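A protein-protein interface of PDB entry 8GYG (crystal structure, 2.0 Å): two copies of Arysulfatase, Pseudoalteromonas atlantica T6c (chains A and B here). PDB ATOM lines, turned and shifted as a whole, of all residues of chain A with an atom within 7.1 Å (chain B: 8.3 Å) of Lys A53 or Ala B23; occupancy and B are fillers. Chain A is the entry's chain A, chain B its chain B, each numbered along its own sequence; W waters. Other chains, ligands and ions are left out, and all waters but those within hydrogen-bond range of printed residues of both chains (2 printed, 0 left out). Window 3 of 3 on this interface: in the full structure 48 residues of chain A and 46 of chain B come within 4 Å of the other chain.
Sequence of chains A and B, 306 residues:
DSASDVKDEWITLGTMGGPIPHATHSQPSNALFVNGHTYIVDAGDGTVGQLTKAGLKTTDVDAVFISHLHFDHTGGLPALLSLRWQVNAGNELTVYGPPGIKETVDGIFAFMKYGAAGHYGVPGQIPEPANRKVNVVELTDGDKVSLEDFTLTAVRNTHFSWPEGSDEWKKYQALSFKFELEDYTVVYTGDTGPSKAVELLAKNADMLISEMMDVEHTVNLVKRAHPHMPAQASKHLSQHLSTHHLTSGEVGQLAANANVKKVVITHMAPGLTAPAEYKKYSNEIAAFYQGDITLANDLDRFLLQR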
ATOM      1  N   LEU A  13       9.483  -0.066  10.338  1.00  0.00           N
ATOM      2  CA  LEU A  13       9.143   1.321  10.654  1.00  0.00           C
ATOM      3  C   LEU A  13       8.751   2.113   9.409  1.00  0.00           C
ATOM      4  O   LEU A  13       7.753   2.854   9.416  1.00  0.00           O
ATOM      5  CB  LEU A  13      10.328   1.995  11.359  1.00  0.00           C
ATOM      6  CG  LEU A  13      10.830   1.445  12.697  1.00  0.00           C
ATOM      7  CD1 LEU A  13      12.090   2.219  13.125  1.00  0.00           C
ATOM      8  CD2 LEU A  13       9.732   1.471  13.788  1.00  0.00           C
ATOM      9  N   SER A  26       6.454   5.127   4.968  1.00  0.00           N
ATOM     10  CA  SER A  26       7.613   5.938   5.307  1.00  0.00           C
ATOM     11  C   SER A  26       8.867   5.345   4.662  1.00  0.00           C
ATOM     12  O   SER A  26       8.871   4.203   4.190  1.00  0.00           O
ATOM     13  CB  SER A  26       7.757   6.035   6.834  1.00  0.00           C
ATOM     14  OG  SER A  26       8.571   7.130   7.236  1.00  0.00           O
ATOM     15  N   THR A  47      13.288   8.133  10.458  1.00  0.00           N
ATOM     16  CA  THR A  47      13.542   6.997  11.338  1.00  0.00           C
ATOM     17  C   THR A  47      13.348   7.371  12.808  1.00  0.00           C
ATOM     18  O   THR A  47      12.810   6.576  13.592  1.00  0.00           O
ATOM     19  CB  THR A  47      14.953   6.480  11.067  1.00  0.00           C
ATOM     20  OG1 THR A  47      14.957   5.867   9.769  1.00  0.00           O
ATOM     21  CG2 THR A  47      15.384   5.490  12.121  1.00  0.00           C
ATOM     22  N   VAL A  48      13.748   8.589  13.191  1.00  0.00           N
ATOM     23  CA  VAL A  48      13.567   9.053  14.568  1.00  0.00           C
ATOM     24  C   VAL A  48      12.086   9.197  14.896  1.00  0.00           C
ATOM     25  O   VAL A  48      11.631   8.795  15.976  1.00  0.00           O
ATOM     26  CB  VAL A  48      14.321  10.382  14.787  1.00  0.00           C
ATOM     27  CG1 VAL A  48      13.872  11.048  16.105  1.00  0.00           C
ATOM     28  CG2 VAL A  48      15.839  10.169  14.773  1.00  0.00           C
ATOM     29  N   GLY A  49      11.314   9.793  13.988  1.00  0.00           N
ATOM     30  CA  GLY A  49       9.873   9.898  14.218  1.00  0.00           C
ATOM     31  C   GLY A  49       9.195   8.541  14.292  1.00  0.00           C
ATOM     32  O   GLY A  49       8.310   8.317  15.125  1.00  0.00           O
ATOM     33  N   GLN A  50       9.624   7.607  13.440  1.00  0.00           N
ATOM     34  CA  GLN A  50       8.943   6.317  13.353  1.00  0.00           C
ATOM     35  C   GLN A  50       9.272   5.425  14.549  1.00  0.00           C
ATOM     36  O   GLN A  50       8.375   4.777  15.099  1.00  0.00           O
ATOM     37  CB  GLN A  50       9.288   5.617  12.031  1.00  0.00           C
ATOM     38  CG  GLN A  50       8.762   6.340  10.782  1.00  0.00           C
ATOM     39  CD  GLN A  50       7.234   6.449  10.750  1.00  0.00           C
ATOM     40  OE1 GLN A  50       6.661   7.534  10.906  1.00  0.00           O
ATOM     41  NE2 GLN A  50       6.571   5.316  10.568  1.00  0.00           N
ATOM     42  N   LEU A  51      10.538   5.380  14.982  1.00  0.00           N
ATOM     43  CA  LEU A  51      10.859   4.562  16.154  1.00  0.00           C
ATOM     44  C   LEU A  51      10.125   5.072  17.395  1.00  0.00           C
ATOM     45  O   LEU A  51       9.755   4.278  18.271  1.00  0.00           O
ATOM     46  CB  LEU A  51      12.383   4.506  16.381  1.00  0.00           C
ATOM     47  CG  LEU A  51      13.193   5.699  16.899  1.00  0.00           C
ATOM     48  CD1 LEU A  51      13.107   5.855  18.429  1.00  0.00           C
ATOM     49  CD2 LEU A  51      14.682   5.642  16.432  1.00  0.00           C
ATOM     50  N   THR A  52       9.895   6.390  17.477  1.00  0.00           N
ATOM     51  CA  THR A  52       9.131   6.954  18.587  1.00  0.00           C
ATOM     52  C   THR A  52       7.671   6.526  18.517  1.00  0.00           C
ATOM     53  O   THR A  52       7.059   6.200  19.536  1.00  0.00           O
ATOM     54  CB  THR A  52       9.246   8.478  18.567  1.00  0.00           C
ATOM     55  OG1 THR A  52      10.629   8.837  18.490  1.00  0.00           O
ATOM     56  CG2 THR A  52       8.610   9.100  19.815  1.00  0.00           C
ATOM     57  N   LYS A  53       7.096   6.506  17.322  1.00  0.00           N
ATOM     58  CA  LYS A  53       5.730   6.015  17.180  1.00  0.00           C
ATOM     59  C   LYS A  53       5.624   4.552  17.569  1.00  0.00           C
ATOM     60  O   LYS A  53       4.601   4.118  18.108  1.00  0.00           O
ATOM     61  CB  LYS A  53       5.253   6.213  15.749  1.00  0.00           C
ATOM     62  CG  LYS A  53       4.925   7.646  15.429  1.00  0.00           C
ATOM     63  CD  LYS A  53       4.551   7.761  13.975  1.00  0.00           C
ATOM     64  CE  LYS A  53       4.326   9.191  13.573  1.00  0.00           C
ATOM     65  NZ  LYS A  53       4.095   9.216  12.107  1.00  0.00           N
ATOM     66  N   ALA A  54       6.662   3.774  17.292  1.00  0.00           N
ATOM     67  CA  ALA A  54       6.705   2.382  17.709  1.00  0.00           C
ATOM     68  C   ALA A  54       7.007   2.212  19.203  1.00  0.00           C
ATOM     69  O   ALA A  54       7.276   1.084  19.630  1.00  0.00           O
ATOM     70  CB  ALA A  54       7.749   1.619  16.885  1.00  0.00           C
ATOM     71  N   GLY A  55       6.980   3.286  19.995  1.00  0.00           N
ATOM     72  CA  GLY A  55       7.201   3.172  21.429  1.00  0.00           C
ATOM     73  C   GLY A  55       8.643   3.019  21.838  1.00  0.00           C
ATOM     74  O   GLY A  55       8.912   2.689  22.998  1.00  0.00           O
ATOM     75  N   LEU A  56       9.585   3.267  20.933  1.00  0.00           N
ATOM     76  CA  LEU A  56      11.005   3.176  21.228  1.00  0.00           C
ATOM     77  C   LEU A  56      11.578   4.570  21.469  1.00  0.00           C
ATOM     78  O   LEU A  56      10.922   5.585  21.238  1.00  0.00           O
ATOM     79  CB  LEU A  56      11.735   2.470  20.079  1.00  0.00           C
ATOM     80  CG  LEU A  56      11.247   1.049  19.781  1.00  0.00           C
ATOM     81  CD1 LEU A  56      11.961   0.487  18.571  1.00  0.00           C
ATOM     82  CD2 LEU A  56      11.462   0.162  20.991  1.00  0.00           C
ATOM     83  N   LEU A 299       5.110   0.344  11.005  1.00  0.00           N
ATOM     84  CA  LEU A 299       4.970   0.060  12.434  1.00  0.00           C
ATOM     85  C   LEU A 299       4.483  -1.359  12.721  1.00  0.00           C
ATOM     86  O   LEU A 299       4.107  -1.635  13.860  1.00  0.00           O
ATOM     87  CB  LEU A 299       4.044   1.063  13.139  1.00  0.00           C
ATOM     88  CG  LEU A 299       4.350   2.559  12.967  1.00  0.00           C
ATOM     89  CD1 LEU A 299       3.411   3.441  13.793  1.00  0.00           C
ATOM     90  CD2 LEU A 299       5.794   2.861  13.311  1.00  0.00           C
ATOM     91  N   ARG A 301       4.849  -5.200  13.748  1.00  0.00           N
ATOM     92  CA  ARG A 301       5.813  -5.855  14.625  1.00  0.00           C
ATOM     93  C   ARG A 301       5.786  -7.362  14.399  1.00  0.00           C
ATOM     94  O   ARG A 301       4.719  -7.962  14.234  1.00  0.00           O
ATOM     95  CB  ARG A 301       5.534  -5.529  16.094  1.00  0.00           C
ATOM     96  CG  ARG A 301       5.169  -4.069  16.323  1.00  0.00           C
ATOM     97  CD  ARG A 301       4.625  -3.842  17.727  1.00  0.00           C
ATOM     98  NE  ARG A 301       5.676  -3.983  18.729  1.00  0.00           N
ATOM     99  CZ  ARG A 301       6.398  -2.971  19.198  1.00  0.00           C
ATOM    100  NH1 ARG A 301       6.175  -1.734  18.766  1.00  0.00           N
ATOM    101  NH2 ARG A 301       7.346  -3.195  20.105  1.00  0.00           N
ATOM    102  N   MET B  16       6.106  19.543  17.158  1.00  0.00           N
ATOM    103  CA  MET B  16       6.822  19.315  18.405  1.00  0.00           C
ATOM    104  C   MET B  16       7.801  20.442  18.716  1.00  0.00           C
ATOM    105  O   MET B  16       8.467  20.967  17.824  1.00  0.00           O
ATOM    106  CB  MET B  16       7.607  17.996  18.350  1.00  0.00           C
ATOM    107  CG  MET B  16       8.301  17.648  19.658  1.00  0.00           C
ATOM    108  SD  MET B  16       7.058  17.587  20.973  1.00  0.00           S
ATOM    109  CE  MET B  16       8.034  17.548  22.471  1.00  0.00           C
ATOM    110  N   ILE B  20      13.477  16.205  21.897  1.00  0.00           N
ATOM    111  CA  ILE B  20      12.910  14.961  22.417  1.00  0.00           C
ATOM    112  C   ILE B  20      11.715  14.581  21.557  1.00  0.00           C
ATOM    113  O   ILE B  20      10.662  15.231  21.651  1.00  0.00           O
ATOM    114  CB  ILE B  20      12.447  15.073  23.879  1.00  0.00           C
ATOM    115  CG1 ILE B  20      13.506  15.686  24.771  1.00  0.00           C
ATOM    116  CG2 ILE B  20      12.052  13.710  24.405  1.00  0.00           C
ATOM    117  CD1 ILE B  20      13.083  15.692  26.249  1.00  0.00           C
ATOM    118  N   PRO B  21      11.812  13.526  20.754  1.00  0.00           N
ATOM    119  CA  PRO B  21      10.721  13.199  19.832  1.00  0.00           C
ATOM    120  C   PRO B  21       9.451  12.786  20.567  1.00  0.00           C
ATOM    121  O   PRO B  21       9.481  12.286  21.697  1.00  0.00           O
ATOM    122  CB  PRO B  21      11.288  12.031  19.010  1.00  0.00           C
ATOM    123  CG  PRO B  21      12.783  12.030  19.284  1.00  0.00           C
ATOM    124  CD  PRO B  21      12.905  12.544  20.683  1.00  0.00           C
ATOM    125  N   HIS B  22       8.318  13.012  19.897  1.00  0.00           N
ATOM    126  CA  HIS B  22       7.000  12.666  20.415  1.00  0.00           C
ATOM    127  C   HIS B  22       6.285  11.815  19.381  1.00  0.00           C
ATOM    128  O   HIS B  22       6.480  12.002  18.174  1.00  0.00           O
ATOM    129  CB  HIS B  22       6.191  13.931  20.731  1.00  0.00           C
ATOM    130  CG  HIS B  22       4.992  13.696  21.598  1.00  0.00           C
ATOM    131  ND1 HIS B  22       3.767  13.328  21.093  1.00  0.00           N
ATOM    132  CD2 HIS B  22       4.824  13.816  22.938  1.00  0.00           C
ATOM    133  CE1 HIS B  22       2.899  13.213  22.084  1.00  0.00           C
ATOM    134  NE2 HIS B  22       3.516  13.502  23.214  1.00  0.00           N
ATOM    135  N   ALA B  23       5.476  10.860  19.860  1.00  0.00           N
ATOM    136  CA  ALA B  23       4.773   9.948  18.957  1.00  0.00           C
ATOM    137  C   ALA B  23       3.774  10.666  18.048  1.00  0.00           C
ATOM    138  O   ALA B  23       3.561  10.239  16.906  1.00  0.00           O
ATOM    139  CB  ALA B  23       4.062   8.862  19.766  1.00  0.00           C
ATOM    140  N   THR B  24       3.147  11.744  18.515  1.00  0.00           N
ATOM    141  CA  THR B  24       2.082  12.375  17.741  1.00  0.00           C
ATOM    142  C   THR B  24       2.406  13.807  17.333  1.00  0.00           C
ATOM    143  O   THR B  24       1.522  14.502  16.824  1.00  0.00           O
ATOM    144  CB  THR B  24       0.752  12.324  18.513  1.00  0.00           C
ATOM    145  OG1 THR B  24       0.950  12.749  19.860  1.00  0.00           O
ATOM    146  CG2 THR B  24       0.235  10.919  18.543  1.00  0.00           C
ATOM    147  N   HIS B  25       3.649  14.260  17.522  1.00  0.00           N
ATOM    148  CA  HIS B  25       4.079  15.590  17.081  1.00  0.00           C
ATOM    149  C   HIS B  25       5.455  15.416  16.444  1.00  0.00           C
ATOM    150  O   HIS B  25       6.446  15.263  17.146  1.00  0.00           O
ATOM    151  CB  HIS B  25       4.118  16.592  18.235  1.00  0.00           C
ATOM    152  CG  HIS B  25       2.791  16.798  18.910  1.00  0.00           C
ATOM    153  ND1 HIS B  25       1.838  17.673  18.436  1.00  0.00           N
ATOM    154  CD2 HIS B  25       2.277  16.272  20.049  1.00  0.00           C
ATOM    155  CE1 HIS B  25       0.781  17.649  19.229  1.00  0.00           C
ATOM    156  NE2 HIS B  25       1.022  16.806  20.216  1.00  0.00           N
ATOM    157  N   SER B  26       5.499  15.403  15.122  1.00  0.00           N
ATOM    158  CA  SER B  26       6.748  15.277  14.381  1.00  0.00           C
ATOM    159  C   SER B  26       7.613  16.523  14.599  1.00  0.00           C
ATOM    160  O   SER B  26       7.145  17.568  15.049  1.00  0.00           O
ATOM    161  CB  SER B  26       6.444  15.068  12.893  1.00  0.00           C
ATOM    162  OG  SER B  26       7.588  14.715  12.124  1.00  0.00           O
ATOM    163  N   GLY B  49       8.860  13.250   4.864  1.00  0.00           N
ATOM    164  CA  GLY B  49       7.688  12.407   5.066  1.00  0.00           C
ATOM    165  C   GLY B  49       6.415  13.209   5.293  1.00  0.00           C
ATOM    166  O   GLY B  49       5.334  12.818   4.843  1.00  0.00           O
ATOM    167  N   GLN B  50       6.525  14.338   6.002  1.00  0.00           N
ATOM    168  CA  GLN B  50       5.345  15.125   6.359  1.00  0.00           C
ATOM    169  C   GLN B  50       4.835  15.940   5.185  1.00  0.00           C
ATOM    170  O   GLN B  50       3.623  16.103   5.024  1.00  0.00           O
ATOM    171  CB  GLN B  50       5.661  16.047   7.542  1.00  0.00           C
ATOM    172  CG  GLN B  50       5.964  15.318   8.858  1.00  0.00           C
ATOM    173  CD  GLN B  50       4.826  14.438   9.297  1.00  0.00           C
ATOM    174  OE1 GLN B  50       4.929  13.210   9.253  1.00  0.00           O
ATOM    175  NE2 GLN B  50       3.724  15.056   9.726  1.00  0.00           N
ATOM    176  N   LYS B  53       2.843  13.599   3.133  1.00  0.00           N
ATOM    177  CA  LYS B  53       1.536  13.410   3.761  1.00  0.00           C
ATOM    178  C   LYS B  53       0.617  14.601   3.513  1.00  0.00           C
ATOM    179  O   LYS B  53      -0.608  14.440   3.416  1.00  0.00           O
ATOM    180  CB  LYS B  53       1.709  13.204   5.272  1.00  0.00           C
ATOM    181  CG  LYS B  53       2.160  11.816   5.664  1.00  0.00           C
ATOM    182  CD  LYS B  53       2.100  11.692   7.180  1.00  0.00           C
ATOM    183  CE  LYS B  53       3.171  10.781   7.710  1.00  0.00           C
ATOM    184  NZ  LYS B  53       3.170  10.754   9.221  1.00  0.00           N
ATOM    185  N   GLY B 271       4.826  17.814  24.171  1.00  0.00           N
ATOM    186  CA  GLY B 271       3.719  17.595  23.253  1.00  0.00           C
ATOM    187  C   GLY B 271       2.425  17.413  24.027  1.00  0.00           C
ATOM    188  O   GLY B 271       2.416  16.883  25.136  1.00  0.00           O
ATOM    189  N   THR B 273      -1.564  16.007  24.417  1.00  0.00           N
ATOM    190  CA  THR B 273      -2.333  14.821  24.021  1.00  0.00           C
ATOM    191  C   THR B 273      -3.772  14.791  24.516  1.00  0.00           C
ATOM    192  O   THR B 273      -4.514  13.893  24.101  1.00  0.00           O
ATOM    193  CB  THR B 273      -1.641  13.522  24.497  1.00  0.00           C
ATOM    194  OG1 THR B 273      -1.490  13.528  25.925  1.00  0.00           O
ATOM    195  CG2 THR B 273      -0.271  13.344  23.832  1.00  0.00           C
ATOM    196  N   ASP B 298      -0.074  18.415  13.645  1.00  0.00           N
ATOM    197  CA  ASP B 298       0.618  17.987  12.435  1.00  0.00           C
ATOM    198  C   ASP B 298      -0.344  17.924  11.276  1.00  0.00           C
ATOM    199  O   ASP B 298      -1.360  17.228  11.349  1.00  0.00           O
ATOM    200  CB  ASP B 298       1.248  16.600  12.639  1.00  0.00           C
ATOM    201  CG  ASP B 298       2.485  16.628  13.531  1.00  0.00           C
ATOM    202  OD1 ASP B 298       2.784  17.703  14.075  1.00  0.00           O
ATOM    203  OD2 ASP B 298       3.152  15.567  13.691  1.00  0.00           O
ATOM    204  N   LEU B 299      -0.019  18.644  10.203  1.00  0.00           N
ATOM    205  CA  LEU B 299      -0.667  18.626   8.905  1.00  0.00           C
ATOM    206  C   LEU B 299      -1.855  19.586   8.875  1.00  0.00           C
ATOM    207  O   LEU B 299      -2.483  19.728   7.820  1.00  0.00           O
ATOM    208  CB  LEU B 299      -1.116  17.218   8.481  1.00  0.00           C
ATOM    209  CG  LEU B 299       0.002  16.168   8.548  1.00  0.00           C
ATOM    210  CD1 LEU B 299      -0.490  14.783   8.182  1.00  0.00           C
ATOM    211  CD2 LEU B 299       1.162  16.573   7.640  1.00  0.00           C
HETATM  212  O   HOH W   1       4.799   8.614   9.204  1.00  0.00           O
HETATM  213  O   HOH W   2       6.937  10.974  15.682  1.00  0.00           O
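NZ of Lys B53 lies close to NZ of Lys A53 (3.4 Å).
The backbone carbonyl oxygen (O) of Val A48 lies within hydrogen-bond range of the side-chain hydroxyl (OG1) of Thr A52, 2.7 Å away.
OE1 of Gln B50 lies within hydrogen-bond range of NZ of Lys B53 (3.0 Å).
OE1 of Gln A50 lies within hydrogen-bond range of NZ of Lys A53 (3.3 Å).
ND1 of His B22 is in hydrogen-bond range of N of Thr B24, 3.1 Å away.
Among the printed residues, pairs that only touch across the chains: Lys A53 with Ala B23 (3.3 Å), Thr A52 with Pro B21 (3.3 Å), Val A48 with Pro B21 (3.5 Å), Thr A52 with Ala B23 (3.6 Å) and Thr A52 with His B22 (3.6 Å).
Of chain B, only Ala B23 (3.3 Å) and Lys B53 (3.4 Å) come within 4 Å of Lys A53.
Of chain A, only Thr A52 (3.6 Å) and Lys A53 (3.3 Å) come within 4 Å of Ala B23.
Of the printed residues of chain B, Thr A52 touches Pro B21, His B22 and Ala B23.
Printed residues of chain A within 4 Å of Lys B53: Lys A53.
Ala A54 touches none of the printed residues of chain B.
Gly B49 touches none of the printed residues of chain A.
The nearest residue of chain B that does not touch Lys A53 is Gln B50 (5.0 Å).
The nearest residue of chain A that does not touch Ala B23 is Gly A49 (5.4 Å).
Of the 15 printed residues of chain B, 4 touch a printed residue of chain A.
Printed residues of chain B that touch a printed residue of chain A: Pro B21, His B22, Ala B23 and Lys B53.
Hydrophobic or aromatic side chains of chain B within 4 Å of the printed part of chain A: Pro B21.
Of the 14 printed residues of chain A, 3 touch a printed residue of chain B.
Printed residues of chain A that touch a printed residue of chain B: Val A48, Thr A52 and Lys A53.
Hydrophobic or aromatic side chains of chain A within 4 Å of the printed part of chain B: Val A48.
Among the printed residues, 6 pairs touch across the chains.
Among the printed residues, no Asp or Glu carboxylate lies within 4 Å of a Lys or Arg side-chain nitrogen of the other chain.
Lys A53 touches its own counterpart, Lys B53.
Positions printed for both chains: 26, 49, 50, 53 and 299.
Of the 6 pairs that touch across the chains among the printed residues, 1 has its exchanged pair printed and touching as well.
Water W1 lies within hydrogen-bond range of the side-chain amino group of Lys B53 (2.7 Å), the side-chain amide oxygen of Gln A50 (2.7 Å) and the side-chain amino group of Lys A53 (3.0 Å).
Water W2 bridges O of His B22 (2.7 Å) and O of Gly A49 (3.0 Å).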
